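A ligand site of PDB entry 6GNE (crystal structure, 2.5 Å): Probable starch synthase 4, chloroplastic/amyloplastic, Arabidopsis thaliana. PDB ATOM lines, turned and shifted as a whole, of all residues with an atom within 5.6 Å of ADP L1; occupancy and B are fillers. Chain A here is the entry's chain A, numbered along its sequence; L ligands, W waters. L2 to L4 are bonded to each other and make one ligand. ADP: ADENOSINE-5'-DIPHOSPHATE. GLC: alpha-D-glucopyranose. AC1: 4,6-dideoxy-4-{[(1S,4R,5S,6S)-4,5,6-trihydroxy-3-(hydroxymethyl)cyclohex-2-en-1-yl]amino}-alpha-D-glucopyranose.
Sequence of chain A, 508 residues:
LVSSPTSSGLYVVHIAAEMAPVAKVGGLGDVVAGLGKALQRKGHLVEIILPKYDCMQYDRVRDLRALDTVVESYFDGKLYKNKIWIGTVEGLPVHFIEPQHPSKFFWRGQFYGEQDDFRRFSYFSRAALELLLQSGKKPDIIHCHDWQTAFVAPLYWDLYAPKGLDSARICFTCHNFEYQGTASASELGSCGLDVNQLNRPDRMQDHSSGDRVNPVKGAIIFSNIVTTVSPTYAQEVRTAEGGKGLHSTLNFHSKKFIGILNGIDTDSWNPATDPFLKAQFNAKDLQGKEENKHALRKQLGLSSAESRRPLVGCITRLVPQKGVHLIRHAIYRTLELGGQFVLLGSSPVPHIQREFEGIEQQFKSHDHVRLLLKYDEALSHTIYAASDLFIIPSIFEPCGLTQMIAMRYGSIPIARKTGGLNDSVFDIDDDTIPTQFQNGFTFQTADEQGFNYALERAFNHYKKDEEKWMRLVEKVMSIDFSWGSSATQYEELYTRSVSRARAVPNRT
The side-chain amino group of Lys 24 is in salt-bridge range of the side-chain carboxylate of Asp 30 (2.7 Å). The backbone NH (N) of Leu 401 sits at hydrogen-bond distance from the side-chain amide oxygen (OE1) of Gln 403. NZ of Lys 322 is in salt-bridge range of OE1 of Glu 397 (2.8 Å). The side-chain carboxylate of Asp 376 is in salt-bridge range of the side-chain amino group of Lys 374, 3.6 Å away. N of Lys 374 lies within hydrogen-bond range of O of Gly 345. The backbone NH (N) of Thr 316 sits at hydrogen-bond distance from the backbone carbonyl oxygen (O) of Leu 344, 3.1 Å away. NE2 of Gln 403 lies within hydrogen-bond range of O of Gly 400, at 3.0 Å. The backbone carbonyl oxygen of Glu 377 is in hydrogen-bond range of the side-chain hydroxyl of Ser 380, 2.8 Å away.
Merely in contact with ADP L1: Tyr 375 (3.3 Å), Thr 316 (3.4 Å), Gly 345 (3.5 Å), Gly 400 (3.5 Å), Ile 315 (3.7 Å), Leu 344 (3.8 Å), Gly 26 (3.8 Å), Ile 405 (3.9 Å) and Ser 380 (3.96 Å). Hydrophobic or aromatic side chains within 4 Å of ADP L1: Ile 315, Leu 344, Tyr 375, Tyr 384, Leu 401 and Ile 405. Within 4 Å of ADP L1: Lys 24, Gly 26, Gly 27, Asp 30, Ile 315, Thr 316, Arg 317, Lys 322, Leu 344, Gly 345, Lys 374, Tyr 375, Asp 376, Ser 380, Tyr 384, Gly 400, Leu 401, Thr 402 and Ile 405. The nearest printed residue that does not touch ADP L1 is Gln 321 (4.003 Å).
O3B of ADP L1 is in hydrogen-bond range of O2B of AC1 L4 (2.6 Å).
Water W3 lies within hydrogen-bond range of an oxygen (O2B) of ADP L1 (2.7 Å) and the backbone NH of Arg 317 (3.2 Å). Water W1 bridges the side-chain hydroxyl (OG) of Ser 380 (2.7 Å) and an oxygen (O2') of ADP L1 (2.7 Å). Water W4 lies within hydrogen-bond range of N6 of ADP L1, O of Thr 316 and N of Ser 346. Water W2 lies within hydrogen-bond range of an oxygen (O1A) of ADP L1 and the side-chain amino group of Lys 322.
O2' of ADP L1 sits at hydrogen-bond distance from OH of Tyr 384 (2.7 Å). NE of Arg 317 lies within salt-bridge range of O2B of ADP L1 (2.7 Å). The side-chain carboxylate of Asp 30 lies within hydrogen-bond range of an oxygen (O3') of ADP L1. The backbone NH (N) of Leu 401 is in hydrogen-bond range of an oxygen (O1A) of ADP L1. O3B of ADP L1 is in salt-bridge range of NZ of Lys 322 (2.9 Å). N of Gly 27 lies within hydrogen-bond range of O1B of ADP L1. A nitrogen (N6) of ADP L1 is in hydrogen-bond range of the backbone carbonyl oxygen of Lys 374 (3.0 Å). NZ of Lys 24 is in hydrogen-bond range of O3' of ADP L1 (3.0 Å). The backbone NH of Asp 376 is in hydrogen-bond range of a nitrogen (N1) of ADP L1. An oxygen (O1A) of ADP L1 is in hydrogen-bond range of the backbone NH (N) of Thr 402 (3.5 Å). NH1 of Arg 317 sits at hydrogen-bond distance from O6 of GLC L3 (3.5 Å). The backbone NH (N) of Gly 400 sits at hydrogen-bond distance from an oxygen (O4) of AC1 L4 (2.9 Å). O2B of AC1 L4 sits at hydrogen-bond distance from NE2 of Gln 321 (2.9 Å). OE1 of Glu 397 sits at hydrogen-bond distance from O3B of AC1 L4 (2.7 Å). N of Cys 399 lies within hydrogen-bond range of O3B of AC1 L4, at 3.1 Å.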
ATOM      1  N   LYS A  24       7.521   7.638  17.866  1.00  0.00           N
ATOM      2  CA  LYS A  24       7.495   7.940  16.461  1.00  0.00           C
ATOM      3  C   LYS A  24       7.767   9.413  16.165  1.00  0.00           C
ATOM      4  O   LYS A  24       7.116  10.301  16.725  1.00  0.00           O
ATOM      5  CB  LYS A  24       6.137   7.595  15.890  1.00  0.00           C
ATOM      6  CG  LYS A  24       6.027   7.954  14.418  1.00  0.00           C
ATOM      7  CD  LYS A  24       4.634   7.803  13.901  1.00  0.00           C
ATOM      8  CE  LYS A  24       4.590   8.218  12.439  1.00  0.00           C
ATOM      9  NZ  LYS A  24       3.436   7.611  11.733  1.00  0.00           N
ATOM     10  N   VAL A  25       8.703   9.630  15.234  1.00  0.00           N
ATOM     11  CA  VAL A  25       8.982  10.953  14.673  1.00  0.00           C
ATOM     12  C   VAL A  25       8.582  11.000  13.193  1.00  0.00           C
ATOM     13  O   VAL A  25       7.965  11.960  12.756  1.00  0.00           O
ATOM     14  CB  VAL A  25      10.474  11.324  14.853  1.00  0.00           C
ATOM     15  CG1 VAL A  25      10.816  12.615  14.076  1.00  0.00           C
ATOM     16  CG2 VAL A  25      10.795  11.473  16.339  1.00  0.00           C
ATOM     17  N   GLY A  26       8.989  10.013  12.413  1.00  0.00           N
ATOM     18  CA  GLY A  26       8.497   9.879  11.060  1.00  0.00           C
ATOM     19  C   GLY A  26       8.393   8.454  10.588  1.00  0.00           C
ATOM     20  O   GLY A  26       7.894   7.587  11.289  1.00  0.00           O
ATOM     21  N   GLY A  27       8.883   8.208   9.374  1.00  0.00           N
ATOM     22  CA  GLY A  27       8.708   6.946   8.727  1.00  0.00           C
ATOM     23  C   GLY A  27       9.484   5.772   9.308  1.00  0.00           C
ATOM     24  O   GLY A  27       9.080   4.628   9.123  1.00  0.00           O
ATOM     25  N   LEU A  28      10.604   6.057   9.963  1.00  0.00           N
ATOM     26  CA  LEU A  28      11.443   5.011  10.549  1.00  0.00           C
ATOM     27  C   LEU A  28      10.632   4.204  11.538  1.00  0.00           C
ATOM     28  O   LEU A  28      10.531   2.994  11.449  1.00  0.00           O
ATOM     29  CB  LEU A  28      12.682   5.594  11.232  1.00  0.00           C
ATOM     30  CG  LEU A  28      13.696   4.493  11.626  1.00  0.00           C
ATOM     31  CD1 LEU A  28      15.135   4.898  11.298  1.00  0.00           C
ATOM     32  CD2 LEU A  28      13.563   4.193  13.099  1.00  0.00           C
ATOM     33  N   ASP A  30       7.467   3.953  11.647  1.00  0.00           N
ATOM     34  CA  ASP A  30       6.408   3.227  10.944  1.00  0.00           C
ATOM     35  C   ASP A  30       6.920   1.899  10.397  1.00  0.00           C
ATOM     36  O   ASP A  30       6.242   0.874  10.502  1.00  0.00           O
ATOM     37  CB  ASP A  30       5.846   4.042   9.762  1.00  0.00           C
ATOM     38  CG  ASP A  30       4.863   5.108  10.186  1.00  0.00           C
ATOM     39  OD1 ASP A  30       4.444   5.175  11.362  1.00  0.00           O
ATOM     40  OD2 ASP A  30       4.435   5.875   9.309  1.00  0.00           O
ATOM     41  N   TRP A 269      -3.315   1.305   8.756  1.00  0.00           N
ATOM     42  CA  TRP A 269      -3.751   2.233   7.703  1.00  0.00           C
ATOM     43  C   TRP A 269      -4.779   1.557   6.807  1.00  0.00           C
ATOM     44  O   TRP A 269      -4.430   0.953   5.802  1.00  0.00           O
ATOM     45  CB  TRP A 269      -2.543   2.756   6.942  1.00  0.00           C
ATOM     46  CG  TRP A 269      -1.617   3.539   7.818  1.00  0.00           C
ATOM     47  CD1 TRP A 269      -0.435   3.107   8.375  1.00  0.00           C
ATOM     48  CD2 TRP A 269      -1.804   4.873   8.273  1.00  0.00           C
ATOM     49  NE1 TRP A 269       0.128   4.114   9.140  1.00  0.00           N
ATOM     50  CE2 TRP A 269      -0.709   5.194   9.109  1.00  0.00           C
ATOM     51  CE3 TRP A 269      -2.811   5.818   8.092  1.00  0.00           C
ATOM     52  CZ2 TRP A 269      -0.588   6.436   9.728  1.00  0.00           C
ATOM     53  CZ3 TRP A 269      -2.691   7.040   8.698  1.00  0.00           C
ATOM     54  CH2 TRP A 269      -1.591   7.348   9.501  1.00  0.00           C
ATOM     55  N   ILE A 315       0.702  16.420   4.454  1.00  0.00           N
ATOM     56  CA  ILE A 315       1.090  15.982   5.816  1.00  0.00           C
ATOM     57  C   ILE A 315       2.551  15.641   5.763  1.00  0.00           C
ATOM     58  O   ILE A 315       2.958  14.683   5.095  1.00  0.00           O
ATOM     59  CB  ILE A 315       0.319  14.736   6.249  1.00  0.00           C
ATOM     60  CG1 ILE A 315      -1.170  15.062   6.381  1.00  0.00           C
ATOM     61  CG2 ILE A 315       0.857  14.230   7.577  1.00  0.00           C
ATOM     62  CD1 ILE A 315      -2.064  13.858   6.329  1.00  0.00           C
ATOM     63  N   THR A 316       3.367  16.389   6.494  1.00  0.00           N
ATOM     64  CA  THR A 316       4.809  16.277   6.342  1.00  0.00           C
ATOM     65  C   THR A 316       5.550  17.007   7.457  1.00  0.00           C
ATOM     66  O   THR A 316       4.989  17.861   8.150  1.00  0.00           O
ATOM     67  CB  THR A 316       5.251  16.880   4.991  1.00  0.00           C
ATOM     68  OG1 THR A 316       6.621  16.591   4.741  1.00  0.00           O
ATOM     69  CG2 THR A 316       5.034  18.388   4.962  1.00  0.00           C
ATOM     70  N   ARG A 317       6.808  16.644   7.628  1.00  0.00           N
ATOM     71  CA  ARG A 317       7.724  17.456   8.394  1.00  0.00           C
ATOM     72  C   ARG A 317       8.161  18.525   7.410  1.00  0.00           C
ATOM     73  O   ARG A 317       8.338  18.259   6.247  1.00  0.00           O
ATOM     74  CB  ARG A 317       8.932  16.624   8.900  1.00  0.00           C
ATOM     75  CG  ARG A 317       8.527  15.535   9.909  1.00  0.00           C
ATOM     76  CD  ARG A 317       9.615  14.500  10.244  1.00  0.00           C
ATOM     77  NE  ARG A 317      10.321  14.033   9.040  1.00  0.00           N
ATOM     78  CZ  ARG A 317      11.502  14.484   8.601  1.00  0.00           C
ATOM     79  NH1 ARG A 317      12.136  15.429   9.285  1.00  0.00           N
ATOM     80  NH2 ARG A 317      12.067  13.988   7.480  1.00  0.00           N
ATOM     81  N   GLN A 321      14.272  18.780   2.714  1.00  0.00           N
ATOM     82  CA  GLN A 321      14.100  17.551   1.954  1.00  0.00           C
ATOM     83  C   GLN A 321      12.736  17.486   1.242  1.00  0.00           C
ATOM     84  O   GLN A 321      12.632  16.985   0.088  1.00  0.00           O
ATOM     85  CB  GLN A 321      14.266  16.352   2.876  1.00  0.00           C
ATOM     86  CG  GLN A 321      13.949  14.991   2.251  1.00  0.00           C
ATOM     87  CD  GLN A 321      13.854  13.870   3.259  1.00  0.00           C
ATOM     88  OE1 GLN A 321      14.472  13.947   4.320  1.00  0.00           O
ATOM     89  NE2 GLN A 321      13.072  12.824   2.933  1.00  0.00           N
ATOM     90  N   LYS A 322      11.717  17.993   1.927  1.00  0.00           N
ATOM     91  CA  LYS A 322      10.335  17.859   1.481  1.00  0.00           C
ATOM     92  C   LYS A 322       9.892  18.914   0.442  1.00  0.00           C
ATOM     93  O   LYS A 322       8.726  18.922   0.029  1.00  0.00           O
ATOM     94  CB  LYS A 322       9.426  17.929   2.710  1.00  0.00           C
ATOM     95  CG  LYS A 322       9.738  16.854   3.738  1.00  0.00           C
ATOM     96  CD  LYS A 322       9.457  15.441   3.218  1.00  0.00           C
ATOM     97  CE  LYS A 322       9.558  14.418   4.321  1.00  0.00           C
ATOM     98  NZ  LYS A 322       9.606  13.033   3.825  1.00  0.00           N
ATOM     99  N   LEU A 344      -0.882  19.922   7.301  1.00  0.00           N
ATOM    100  CA  LEU A 344      -0.526  19.489   8.637  1.00  0.00           C
ATOM    101  C   LEU A 344       0.971  19.225   8.647  1.00  0.00           C
ATOM    102  O   LEU A 344       1.440  18.302   7.999  1.00  0.00           O
ATOM    103  CB  LEU A 344      -1.303  18.226   8.991  1.00  0.00           C
ATOM    104  CG  LEU A 344      -0.999  17.578  10.334  1.00  0.00           C
ATOM    105  CD1 LEU A 344      -1.228  18.589  11.438  1.00  0.00           C
ATOM    106  CD2 LEU A 344      -1.908  16.365  10.485  1.00  0.00           C
ATOM    107  N   GLY A 345       1.728  20.047   9.342  1.00  0.00           N
ATOM    108  CA  GLY A 345       3.168  19.845   9.418  1.00  0.00           C
ATOM    109  C   GLY A 345       3.822  20.764  10.408  1.00  0.00           C
ATOM    110  O   GLY A 345       3.294  21.844  10.676  1.00  0.00           O
ATOM    111  N   SER A 346       4.954  20.353  10.964  1.00  0.00           N
ATOM    112  CA  SER A 346       5.794  21.321  11.653  1.00  0.00           C
ATOM    113  C   SER A 346       7.266  21.128  11.351  1.00  0.00           C
ATOM    114  O   SER A 346       7.658  20.100  10.838  1.00  0.00           O
ATOM    115  CB  SER A 346       5.524  21.365  13.170  1.00  0.00           C
ATOM    116  OG  SER A 346       5.803  20.135  13.739  1.00  0.00           O
ATOM    117  N   LYS A 374       1.685  21.687  13.508  1.00  0.00           N
ATOM    118  CA  LYS A 374       1.865  20.788  14.641  1.00  0.00           C
ATOM    119  C   LYS A 374       1.919  19.322  14.178  1.00  0.00           C
ATOM    120  O   LYS A 374       1.529  19.012  13.062  1.00  0.00           O
ATOM    121  CB  LYS A 374       0.707  20.945  15.651  1.00  0.00           C
ATOM    122  CG  LYS A 374      -0.660  20.580  15.075  1.00  0.00           C
ATOM    123  CD  LYS A 374      -1.809  20.962  15.994  1.00  0.00           C
ATOM    124  CE  LYS A 374      -3.070  20.271  15.526  1.00  0.00           C
ATOM    125  NZ  LYS A 374      -4.208  20.633  16.391  1.00  0.00           N
ATOM    126  N   TYR A 375       2.420  18.446  15.053  1.00  0.00           N
ATOM    127  CA  TYR A 375       2.343  17.001  14.892  1.00  0.00           C
ATOM    128  C   TYR A 375       0.996  16.570  15.468  1.00  0.00           C
ATOM    129  O   TYR A 375       0.726  16.908  16.581  1.00  0.00           O
ATOM    130  CB  TYR A 375       3.503  16.270  15.634  1.00  0.00           C
ATOM    131  CG  TYR A 375       3.495  14.818  15.300  1.00  0.00           C
ATOM    132  CD1 TYR A 375       4.075  14.367  14.099  1.00  0.00           C
ATOM    133  CD2 TYR A 375       2.809  13.883  16.112  1.00  0.00           C
ATOM    134  CE1 TYR A 375       4.014  13.025  13.720  1.00  0.00           C
ATOM    135  CE2 TYR A 375       2.730  12.544  15.731  1.00  0.00           C
ATOM    136  CZ  TYR A 375       3.349  12.130  14.535  1.00  0.00           C
ATOM    137  OH  TYR A 375       3.289  10.796  14.143  1.00  0.00           O
ATOM    138  N   ASP A 376       0.151  15.900  14.699  1.00  0.00           N
ATOM    139  CA  ASP A 376      -1.125  15.377  15.232  1.00  0.00           C
ATOM    140  C   ASP A 376      -1.565  14.110  14.484  1.00  0.00           C
ATOM    141  O   ASP A 376      -1.969  14.169  13.315  1.00  0.00           O
ATOM    142  CB  ASP A 376      -2.211  16.462  15.149  1.00  0.00           C
ATOM    143  CG  ASP A 376      -3.497  16.081  15.856  1.00  0.00           C
ATOM    144  OD1 ASP A 376      -3.912  14.912  15.867  1.00  0.00           O
ATOM    145  OD2 ASP A 376      -4.172  16.995  16.372  1.00  0.00           O
ATOM    146  N   GLU A 377      -1.532  12.996  15.199  1.00  0.00           N
ATOM    147  CA  GLU A 377      -1.828  11.680  14.639  1.00  0.00           C
ATOM    148  C   GLU A 377      -3.279  11.559  14.227  1.00  0.00           C
ATOM    149  O   GLU A 377      -3.593  11.247  13.093  1.00  0.00           O
ATOM    150  CB  GLU A 377      -1.492  10.560  15.649  1.00  0.00           C
ATOM    151  CG  GLU A 377      -1.260   9.227  14.938  1.00  0.00           C
ATOM    152  CD  GLU A 377      -1.348   7.984  15.818  1.00  0.00           C
ATOM    153  OE1 GLU A 377      -1.281   6.895  15.211  1.00  0.00           O
ATOM    154  OE2 GLU A 377      -1.459   8.072  17.078  1.00  0.00           O
ATOM    155  N   SER A 380      -4.068  13.606  11.029  1.00  0.00           N
ATOM    156  CA  SER A 380      -3.529  13.019   9.804  1.00  0.00           C
ATOM    157  C   SER A 380      -4.445  11.984   9.198  1.00  0.00           C
ATOM    158  O   SER A 380      -4.701  12.012   7.994  1.00  0.00           O
ATOM    159  CB  SER A 380      -2.105  12.462   9.997  1.00  0.00           C
ATOM    160  OG  SER A 380      -2.093  11.285  10.737  1.00  0.00           O
ATOM    161  N   TYR A 384      -5.904  12.448   5.317  1.00  0.00           N
ATOM    162  CA  TYR A 384      -5.750  11.445   4.243  1.00  0.00           C
ATOM    163  C   TYR A 384      -7.156  11.060   3.726  1.00  0.00           C
ATOM    164  O   TYR A 384      -7.398  11.058   2.521  1.00  0.00           O
ATOM    165  CB  TYR A 384      -5.029  10.177   4.723  1.00  0.00           C
ATOM    166  CG  TYR A 384      -3.537  10.307   5.002  1.00  0.00           C
ATOM    167  CD1 TYR A 384      -2.634  10.654   3.990  1.00  0.00           C
ATOM    168  CD2 TYR A 384      -3.024  10.036   6.275  1.00  0.00           C
ATOM    169  CE1 TYR A 384      -1.266  10.758   4.238  1.00  0.00           C
ATOM    170  CE2 TYR A 384      -1.645  10.144   6.544  1.00  0.00           C
ATOM    171  CZ  TYR A 384      -0.759  10.487   5.518  1.00  0.00           C
ATOM    172  OH  TYR A 384       0.587  10.571   5.801  1.00  0.00           O
ATOM    173  N   GLU A 397      13.877  11.828  -1.599  1.00  0.00           N
ATOM    174  CA  GLU A 397      12.976  11.042  -0.793  1.00  0.00           C
ATOM    175  C   GLU A 397      13.397   9.556  -0.836  1.00  0.00           C
ATOM    176  O   GLU A 397      13.087   8.834  -1.785  1.00  0.00           O
ATOM    177  CB  GLU A 397      11.535  11.246  -1.274  1.00  0.00           C
ATOM    178  CG  GLU A 397      10.473  10.792  -0.290  1.00  0.00           C
ATOM    179  CD  GLU A 397      10.416  11.651   0.965  1.00  0.00           C
ATOM    180  OE1 GLU A 397      10.699  11.121   2.035  1.00  0.00           O
ATOM    181  OE2 GLU A 397      10.089  12.839   0.903  1.00  0.00           O
ATOM    182  N   CYS A 399      12.321   6.928   0.633  1.00  0.00           N
ATOM    183  CA  CYS A 399      11.130   6.180   0.271  1.00  0.00           C
ATOM    184  C   CYS A 399       9.887   7.060   0.265  1.00  0.00           C
ATOM    185  O   CYS A 399       9.280   7.295  -0.788  1.00  0.00           O
ATOM    186  CB  CYS A 399      10.919   4.986   1.168  1.00  0.00           C
ATOM    187  SG  CYS A 399       9.486   3.990   0.669  1.00  0.00           S
ATOM    188  N   GLY A 400       9.491   7.525   1.429  1.00  0.00           N
ATOM    189  CA  GLY A 400       8.226   8.191   1.604  1.00  0.00           C
ATOM    190  C   GLY A 400       7.102   7.168   1.784  1.00  0.00           C
ATOM    191  O   GLY A 400       6.981   6.205   1.015  1.00  0.00           O
ATOM    192  N   LEU A 401       6.310   7.376   2.820  1.00  0.00           N
ATOM    193  CA  LEU A 401       5.173   6.554   3.144  1.00  0.00           C
ATOM    194  C   LEU A 401       3.847   7.279   2.918  1.00  0.00           C
ATOM    195  O   LEU A 401       2.801   6.641   2.662  1.00  0.00           O
ATOM    196  CB  LEU A 401       5.268   6.127   4.595  1.00  0.00           C
ATOM    197  CG  LEU A 401       6.532   5.386   5.014  1.00  0.00           C
ATOM    198  CD1 LEU A 401       6.401   4.966   6.468  1.00  0.00           C
ATOM    199  CD2 LEU A 401       6.796   4.172   4.147  1.00  0.00           C
ATOM    200  N   THR A 402       3.860   8.614   3.009  1.00  0.00           N
ATOM    201  CA  THR A 402       2.629   9.389   2.954  1.00  0.00           C
ATOM    202  C   THR A 402       1.888   9.229   1.613  1.00  0.00           C
ATOM    203  O   THR A 402       0.648   9.231   1.585  1.00  0.00           O
ATOM    204  CB  THR A 402       2.906  10.838   3.217  1.00  0.00           C
ATOM    205  OG1 THR A 402       3.828  11.331   2.226  1.00  0.00           O
ATOM    206  CG2 THR A 402       3.452  11.046   4.658  1.00  0.00           C
ATOM    207  N   GLN A 403       2.630   9.079   0.525  1.00  0.00           N
ATOM    208  CA  GLN A 403       2.003   8.817  -0.775  1.00  0.00           C
ATOM    209  C   GLN A 403       1.308   7.444  -0.820  1.00  0.00           C
ATOM    210  O   GLN A 403       0.286   7.290  -1.480  1.00  0.00           O
ATOM    211  CB  GLN A 403       3.017   8.943  -1.932  1.00  0.00           C
ATOM    212  CG  GLN A 403       3.913   7.726  -2.253  1.00  0.00           C
ATOM    213  CD  GLN A 403       5.146   7.642  -1.382  1.00  0.00           C
ATOM    214  OE1 GLN A 403       5.253   8.306  -0.334  1.00  0.00           O
ATOM    215  NE2 GLN A 403       6.107   6.843  -1.822  1.00  0.00           N
ATOM    216  N   ILE A 405       0.063   5.908   1.972  1.00  0.00           N
ATOM    217  CA  ILE A 405      -1.086   6.057   2.851  1.00  0.00           C
ATOM    218  C   ILE A 405      -2.164   6.835   2.107  1.00  0.00           C
ATOM    219  O   ILE A 405      -3.337   6.420   2.122  1.00  0.00           O
ATOM    220  CB  ILE A 405      -0.754   6.791   4.182  1.00  0.00           C
ATOM    221  CG1 ILE A 405       0.339   6.050   4.986  1.00  0.00           C
ATOM    222  CG2 ILE A 405      -1.986   6.964   5.058  1.00  0.00           C
ATOM    223  CD1 ILE A 405       0.939   6.861   6.103  1.00  0.00           C
HETATM  224  PB  ADP L   1       9.768  11.083   6.841  1.00  0.00           P
HETATM  225  O1B ADP L   1      10.289   9.767   7.359  1.00  0.00           O
HETATM  226  O2B ADP L   1       9.035  11.951   7.818  1.00  0.00           O
HETATM  227  O3B ADP L   1      10.865  11.839   6.124  1.00  0.00           O
HETATM  228  PA  ADP L   1       7.819   9.360   5.576  1.00  0.00           P
HETATM  229  O1A ADP L   1       6.826   9.611   4.478  1.00  0.00           O
HETATM  230  O2A ADP L   1       8.707   8.158   5.375  1.00  0.00           O
HETATM  231  O3A ADP L   1       8.661  10.729   5.721  1.00  0.00           O
HETATM  232  O5' ADP L   1       7.091   9.175   6.992  1.00  0.00           O
HETATM  233  C5' ADP L   1       6.221  10.170   7.544  1.00  0.00           C
HETATM  234  C4' ADP L   1       5.233   9.631   8.600  1.00  0.00           C
HETATM  235  O4' ADP L   1       5.017  10.631   9.614  1.00  0.00           O
HETATM  236  C3' ADP L   1       3.852   9.375   8.034  1.00  0.00           C
HETATM  237  O3' ADP L   1       3.222   8.383   8.841  1.00  0.00           O
HETATM  238  C2' ADP L   1       3.129  10.684   8.231  1.00  0.00           C
HETATM  239  O2' ADP L   1       1.728  10.539   8.274  1.00  0.00           O
HETATM  240  C1' ADP L   1       3.677  11.105   9.564  1.00  0.00           C
HETATM  241  N9  ADP L   1       3.709  12.575   9.753  1.00  0.00           N
HETATM  242  C8  ADP L   1       4.591  13.439   9.256  1.00  0.00           C
HETATM  243  N7  ADP L   1       4.330  14.692   9.683  1.00  0.00           N
HETATM  244  C5  ADP L   1       3.252  14.642  10.486  1.00  0.00           C
HETATM  245  C6  ADP L   1       2.427  15.604  11.275  1.00  0.00           C
HETATM  246  N6  ADP L   1       2.733  16.928  11.276  1.00  0.00           N
HETATM  247  N1  ADP L   1       1.381  15.099  11.983  1.00  0.00           N
HETATM  248  C2  ADP L   1       1.076  13.776  11.958  1.00  0.00           C
HETATM  249  N3  ADP L   1       1.777  12.875  11.260  1.00  0.00           N
HETATM  250  C4  ADP L   1       2.847  13.236  10.513  1.00  0.00           C
HETATM  251  C1  GLC L   2      21.281  18.050  12.437  1.00  0.00           C
HETATM  252  C2  GLC L   2      21.731  16.800  13.225  1.00  0.00           C
HETATM  253  C3  GLC L   2      20.880  15.579  12.878  1.00  0.00           C
HETATM  254  C4  GLC L   2      19.400  15.924  13.143  1.00  0.00           C
HETATM  255  C5  GLC L   2      19.020  17.160  12.320  1.00  0.00           C
HETATM  256  C6  GLC L   2      17.551  17.566  12.515  1.00  0.00           C
HETATM  257  O1  GLC L   2      21.552  17.864  11.040  1.00  0.00           O
HETATM  258  O2  GLC L   2      23.096  16.507  12.921  1.00  0.00           O
HETATM  259  O3  GLC L   2      21.324  14.398  13.584  1.00  0.00           O
HETATM  260  O4  GLC L   2      18.584  14.823  12.743  1.00  0.00           O
HETATM  261  O5  GLC L   2      19.875  18.275  12.649  1.00  0.00           O
HETATM  262  O6  GLC L   2      17.351  17.851  13.899  1.00  0.00           O
HETATM  263  C1  GLC L   3      17.779  14.180  13.703  1.00  0.00           C
HETATM  264  C2  GLC L   3      18.142  12.700  13.817  1.00  0.00           C
HETATM  265  C3  GLC L   3      17.779  11.968  12.526  1.00  0.00           C
HETATM  266  C4  GLC L   3      16.290  12.143  12.275  1.00  0.00           C
HETATM  267  C5  GLC L   3      15.993  13.624  12.135  1.00  0.00           C
HETATM  268  C6  GLC L   3      14.497  13.860  11.964  1.00  0.00           C
HETATM  269  O2  GLC L   3      19.517  12.571  14.144  1.00  0.00           O
HETATM  270  O3  GLC L   3      18.085  10.581  12.618  1.00  0.00           O
HETATM  271  O4  GLC L   3      15.895  11.415  11.109  1.00  0.00           O
HETATM  272  O5  GLC L   3      16.419  14.326  13.313  1.00  0.00           O
HETATM  273  O6  GLC L   3      14.228  15.267  12.050  1.00  0.00           O
HETATM  274  C1  AC1 L   4      15.133  10.235  11.358  1.00  0.00           C
HETATM  275  O2  AC1 L   4      17.012   8.893  10.635  1.00  0.00           O
HETATM  276  C2  AC1 L   4      15.600   9.097  10.454  1.00  0.00           C
HETATM  277  C4A AC1 L   4      11.706   7.137   4.512  1.00  0.00           C
HETATM  278  C3  AC1 L   4      15.225   9.340   8.985  1.00  0.00           C
HETATM  279  O3  AC1 L   4      15.646   8.199   8.235  1.00  0.00           O
HETATM  280  C4  AC1 L   4      13.712   9.590   8.863  1.00  0.00           C
HETATM  281  N4A AC1 L   4      13.226   9.763   7.489  1.00  0.00           N
HETATM  282  C5  AC1 L   4      13.419  10.807   9.745  1.00  0.00           C
HETATM  283  O5  AC1 L   4      13.748  10.497  11.107  1.00  0.00           O
HETATM  284  C6  AC1 L   4      11.953  11.193   9.767  1.00  0.00           C
HETATM  285  C1B AC1 L   4      13.306   8.740   6.435  1.00  0.00           C
HETATM  286  C2B AC1 L   4      13.006   9.263   5.012  1.00  0.00           C
HETATM  287  O2B AC1 L   4      12.927  10.699   4.928  1.00  0.00           O
HETATM  288  C3B AC1 L   4      11.763   8.658   4.364  1.00  0.00           C
HETATM  289  O3B AC1 L   4      11.875   8.906   2.966  1.00  0.00           O
HETATM  290  O4  AC1 L   4      10.476   6.667   3.969  1.00  0.00           O
HETATM  291  C5B AC1 L   4      11.885   6.721   5.939  1.00  0.00           C
HETATM  292  C7B AC1 L   4      12.551   7.474   6.807  1.00  0.00           C
HETATM  293  C6B AC1 L   4      11.345   5.381   6.390  1.00  0.00           C
HETATM  294  O6B AC1 L   4      12.001   4.314   5.690  1.00  0.00           O
HETATM  295  O   HOH W   1       0.377  10.268  10.641  1.00  0.00           O
HETATM  296  O   HOH W   2       6.776  12.442   4.256  1.00  0.00           O
HETATM  297  O   HOH W   3       7.233  13.636   6.683  1.00  0.00           O
HETATM  298  O   HOH W   4       5.528  17.244  10.994  1.00  0.00           O
